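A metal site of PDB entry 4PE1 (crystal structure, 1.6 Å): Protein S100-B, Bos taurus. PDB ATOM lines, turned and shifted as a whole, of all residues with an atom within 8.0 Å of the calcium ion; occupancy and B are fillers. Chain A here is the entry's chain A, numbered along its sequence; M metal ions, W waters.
The calcium ion is bound by OD1 of Asp 62 (2.4 Å), OD1 of Asp 64 (2.4 Å), O of Glu 68 (2.4 Å), OD1 of Asp 66 (2.4 Å), water W1 (2.4 Å), OE1 of Glu 73 (2.4 Å) and OE2 of Glu 73 (2.6 Å).
Five residues have an atom within 4 Å of the calcium ion: Asp 62, Asp 64, Asp 66, Glu 68 and Glu 73.
The nearest printed residue that does not touch the calcium ion is Ser 63 (4.3 Å).
Water W1 bridges OD2 of Asp 70 and OD2 of Asp 64.
N of Gly 65 lies close to OD1 of Asp 62 (3.2 Å).
The side-chain carboxylate (OD2) of Asp 62 is in hydrogen-bond range of the backbone NH (N) of Gly 67 (2.9 Å).
The backbone NH (N) of Ser 63 sits close to the side-chain carboxylate (OE2) of Glu 73, 2.9 Å away.
The backbone NH (N) of Glu 73 sits at hydrogen-bond distance from the side-chain carboxylate (OD1) of Asp 70.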
ATOM      1  N   LYS A  27       6.314   3.836 -11.889  1.00  0.00           N
ATOM      2  CA  LYS A  27       7.742   3.979 -12.185  1.00  0.00           C
ATOM      3  C   LYS A  27       8.176   3.138 -13.382  1.00  0.00           C
ATOM      4  O   LYS A  27       7.542   2.143 -13.731  1.00  0.00           O
ATOM      5  CB  LYS A  27       8.594   3.644 -10.964  1.00  0.00           C
ATOM      6  CG  LYS A  27       8.313   4.506  -9.737  1.00  0.00           C
ATOM      7  CD  LYS A  27       9.130   4.049  -8.557  1.00  0.00           C
ATOM      8  CE  LYS A  27       8.674   4.723  -7.276  1.00  0.00           C
ATOM      9  NZ  LYS A  27       7.204   4.563  -7.085  1.00  0.00           N
ATOM     10  N   LEU A  28       9.254   3.577 -14.043  1.00  0.00           N
ATOM     11  CA  LEU A  28       9.845   2.817 -15.133  1.00  0.00           C
ATOM     12  C   LEU A  28      10.947   1.905 -14.613  1.00  0.00           C
ATOM     13  O   LEU A  28      11.954   2.393 -14.086  1.00  0.00           O
ATOM     14  CB  LEU A  28      10.434   3.762 -16.176  1.00  0.00           C
ATOM     15  CG  LEU A  28       9.469   4.761 -16.818  1.00  0.00           C
ATOM     16  CD1 LEU A  28      10.257   5.890 -17.535  1.00  0.00           C
ATOM     17  CD2 LEU A  28       8.589   4.044 -17.815  1.00  0.00           C
ATOM     18  N   MET A  58      19.970   3.969 -16.588  1.00  0.00           N
ATOM     19  CA  MET A  58      19.179   3.986 -15.357  1.00  0.00           C
ATOM     20  C   MET A  58      19.957   4.603 -14.200  1.00  0.00           C
ATOM     21  O   MET A  58      19.419   5.385 -13.423  1.00  0.00           O
ATOM     22  CB  MET A  58      18.713   2.582 -14.975  1.00  0.00           C
ATOM     23  CG  MET A  58      17.782   2.571 -13.745  1.00  0.00           C
ATOM     24  SD  MET A  58      16.251   3.537 -13.887  1.00  0.00           S
ATOM     25  CE  MET A  58      15.214   2.408 -14.833  1.00  0.00           C
ATOM     26  N   LEU A  61      19.758   8.387 -14.527  1.00  0.00           N
ATOM     27  CA  LEU A  61      18.432   8.951 -14.263  1.00  0.00           C
ATOM     28  C   LEU A  61      17.925   8.737 -12.831  1.00  0.00           C
ATOM     29  O   LEU A  61      17.148   9.540 -12.333  1.00  0.00           O
ATOM     30  CB  LEU A  61      17.403   8.400 -15.260  1.00  0.00           C
ATOM     31  CG  LEU A  61      17.671   8.642 -16.740  1.00  0.00           C
ATOM     32  CD1 LEU A  61      16.488   8.205 -17.585  1.00  0.00           C
ATOM     33  CD2 LEU A  61      17.948  10.130 -16.976  1.00  0.00           C
ATOM     34  N   ASP A  62      18.369   7.652 -12.202  1.00  0.00           N
ATOM     35  CA  ASP A  62      17.834   7.250 -10.896  1.00  0.00           C
ATOM     36  C   ASP A  62      18.546   7.973  -9.743  1.00  0.00           C
ATOM     37  O   ASP A  62      19.684   7.644  -9.400  1.00  0.00           O
ATOM     38  CB  ASP A  62      17.987   5.733 -10.736  1.00  0.00           C
ATOM     39  CG  ASP A  62      17.518   5.244  -9.402  1.00  0.00           C
ATOM     40  OD1 ASP A  62      16.630   5.894  -8.805  1.00  0.00           O
ATOM     41  OD2 ASP A  62      18.039   4.190  -8.941  1.00  0.00           O
ATOM     42  N   SER A  63      17.855   8.950  -9.136  1.00  0.00           N
ATOM     43  CA  SER A  63      18.474   9.767  -8.106  1.00  0.00           C
ATOM     44  C   SER A  63      18.069   9.426  -6.669  1.00  0.00           C
ATOM     45  O   SER A  63      18.642   9.964  -5.722  1.00  0.00           O
ATOM     46  CB  SER A  63      18.233  11.256  -8.398  1.00  0.00           C
ATOM     47  OG  SER A  63      18.932  11.645  -9.561  1.00  0.00           O
ATOM     48  N   ASP A  64      17.103   8.525  -6.491  1.00  0.00           N
ATOM     49  CA  ASP A  64      16.668   8.118  -5.148  1.00  0.00           C
ATOM     50  C   ASP A  64      16.908   6.637  -4.805  1.00  0.00           C
ATOM     51  O   ASP A  64      16.526   6.176  -3.725  1.00  0.00           O
ATOM     52  CB  ASP A  64      15.215   8.521  -4.873  1.00  0.00           C
ATOM     53  CG  ASP A  64      14.229   7.920  -5.871  1.00  0.00           C
ATOM     54  OD1 ASP A  64      14.546   6.901  -6.524  1.00  0.00           O
ATOM     55  OD2 ASP A  64      13.113   8.472  -5.987  1.00  0.00           O
ATOM     56  N   GLY A  65      17.517   5.904  -5.735  1.00  0.00           N
ATOM     57  CA  GLY A  65      18.031   4.577  -5.440  1.00  0.00           C
ATOM     58  C   GLY A  65      17.034   3.442  -5.327  1.00  0.00           C
ATOM     59  O   GLY A  65      17.248   2.513  -4.557  1.00  0.00           O
ATOM     60  N   ASP A  66      15.936   3.503  -6.067  1.00  0.00           N
ATOM     61  CA  ASP A  66      15.043   2.354  -6.110  1.00  0.00           C
ATOM     62  C   ASP A  66      15.304   1.551  -7.370  1.00  0.00           C
ATOM     63  O   ASP A  66      14.608   0.566  -7.659  1.00  0.00           O
ATOM     64  CB  ASP A  66      13.570   2.763  -6.051  1.00  0.00           C
ATOM     65  CG  ASP A  66      13.244   3.899  -6.986  1.00  0.00           C
ATOM     66  OD1 ASP A  66      14.079   4.257  -7.840  1.00  0.00           O
ATOM     67  OD2 ASP A  66      12.112   4.432  -6.856  1.00  0.00           O
ATOM     68  N   GLY A  67      16.304   1.973  -8.146  1.00  0.00           N
ATOM     69  CA  GLY A  67      16.622   1.300  -9.383  1.00  0.00           C
ATOM     70  C   GLY A  67      15.552   1.500 -10.437  1.00  0.00           C
ATOM     71  O   GLY A  67      15.511   0.762 -11.421  1.00  0.00           O
ATOM     72  N   GLU A  68      14.694   2.504 -10.242  1.00  0.00           N
ATOM     73  CA  GLU A  68      13.617   2.791 -11.189  1.00  0.00           C
ATOM     74  C   GLU A  68      13.578   4.276 -11.498  1.00  0.00           C
ATOM     75  O   GLU A  68      14.150   5.096 -10.764  1.00  0.00           O
ATOM     76  CB  GLU A  68      12.244   2.307 -10.674  1.00  0.00           C
ATOM     77  CG  GLU A  68      12.227   0.806 -10.357  1.00  0.00           C
ATOM     78  CD  GLU A  68      10.901   0.108 -10.625  1.00  0.00           C
ATOM     79  OE1 GLU A  68      10.052   0.637 -11.381  1.00  0.00           O
ATOM     80  OE2 GLU A  68      10.710  -1.017 -10.094  1.00  0.00           O
ATOM     81  N   CYS A  69      12.921   4.628 -12.593  1.00  0.00           N
ATOM     82  CA  CYS A  69      12.764   6.030 -12.962  1.00  0.00           C
ATOM     83  C   CYS A  69      11.347   6.452 -12.655  1.00  0.00           C
ATOM     84  O   CYS A  69      10.405   5.968 -13.296  1.00  0.00           O
ATOM     85  CB  CYS A  69      13.072   6.191 -14.459  1.00  0.00           C
ATOM     86  SG  CYS A  69      13.091   7.886 -15.066  1.00  0.00           S
ATOM     87  N   ASP A  70      11.174   7.348 -11.671  1.00  0.00           N
ATOM     88  CA  ASP A  70       9.846   7.866 -11.347  1.00  0.00           C
ATOM     89  C   ASP A  70       9.533   9.065 -12.225  1.00  0.00           C
ATOM     90  O   ASP A  70      10.324   9.382 -13.115  1.00  0.00           O
ATOM     91  CB  ASP A  70       9.688   8.176  -9.854  1.00  0.00           C
ATOM     92  CG  ASP A  70      10.618   9.289  -9.347  1.00  0.00           C
ATOM     93  OD1 ASP A  70      11.078  10.141 -10.131  1.00  0.00           O
ATOM     94  OD2 ASP A  70      10.852   9.339  -8.116  1.00  0.00           O
ATOM     95  N   PHE A  71       8.400   9.718 -12.000  1.00  0.00           N
ATOM     96  CA  PHE A  71       8.010  10.782 -12.911  1.00  0.00           C
ATOM     97  C   PHE A  71       8.935  11.990 -12.839  1.00  0.00           C
ATOM     98  O   PHE A  71       9.272  12.592 -13.869  1.00  0.00           O
ATOM     99  CB  PHE A  71       6.556  11.232 -12.733  1.00  0.00           C
ATOM    100  CG  PHE A  71       6.105  12.142 -13.826  1.00  0.00           C
ATOM    101  CD1 PHE A  71       5.799  11.645 -15.079  1.00  0.00           C
ATOM    102  CD2 PHE A  71       6.060  13.514 -13.625  1.00  0.00           C
ATOM    103  CE1 PHE A  71       5.434  12.484 -16.113  1.00  0.00           C
ATOM    104  CE2 PHE A  71       5.691  14.361 -14.644  1.00  0.00           C
ATOM    105  CZ  PHE A  71       5.360  13.846 -15.886  1.00  0.00           C
ATOM    106  N   GLU A  73      12.079  11.976 -12.145  1.00  0.00           N
ATOM    107  CA  GLU A  73      13.315  11.617 -12.821  1.00  0.00           C
ATOM    108  C   GLU A  73      13.143  11.547 -14.339  1.00  0.00           C
ATOM    109  O   GLU A  73      14.077  11.825 -15.091  1.00  0.00           O
ATOM    110  CB  GLU A  73      13.869  10.295 -12.251  1.00  0.00           C
ATOM    111  CG  GLU A  73      14.319  10.394 -10.775  1.00  0.00           C
ATOM    112  CD  GLU A  73      14.340   9.037 -10.051  1.00  0.00           C
ATOM    113  OE1 GLU A  73      13.773   8.061 -10.584  1.00  0.00           O
ATOM    114  OE2 GLU A  73      14.927   8.957  -8.948  1.00  0.00           O
ATOM    115  N   PHE A  74      11.955  11.170 -14.781  1.00  0.00           N
ATOM    116  CA  PHE A  74      11.662  11.124 -16.209  1.00  0.00           C
ATOM    117  C   PHE A  74      11.603  12.563 -16.738  1.00  0.00           C
ATOM    118  O   PHE A  74      12.089  12.847 -17.845  1.00  0.00           O
ATOM    119  CB  PHE A  74      10.346  10.387 -16.465  1.00  0.00           C
ATOM    120  CG  PHE A  74       9.853  10.470 -17.873  1.00  0.00           C
ATOM    121  CD1 PHE A  74      10.474   9.756 -18.892  1.00  0.00           C
ATOM    122  CD2 PHE A  74       8.747  11.255 -18.190  1.00  0.00           C
ATOM    123  CE1 PHE A  74      10.004   9.819 -20.200  1.00  0.00           C
ATOM    124  CE2 PHE A  74       8.264  11.334 -19.490  1.00  0.00           C
ATOM    125  CZ  PHE A  74       8.901  10.615 -20.509  1.00  0.00           C
HETATM  126 CA    CA M   1      14.336   6.448  -8.832  1.00  0.00          CA
HETATM  127  O   HOH W   1      11.970   6.324  -8.267  1.00  0.00           O
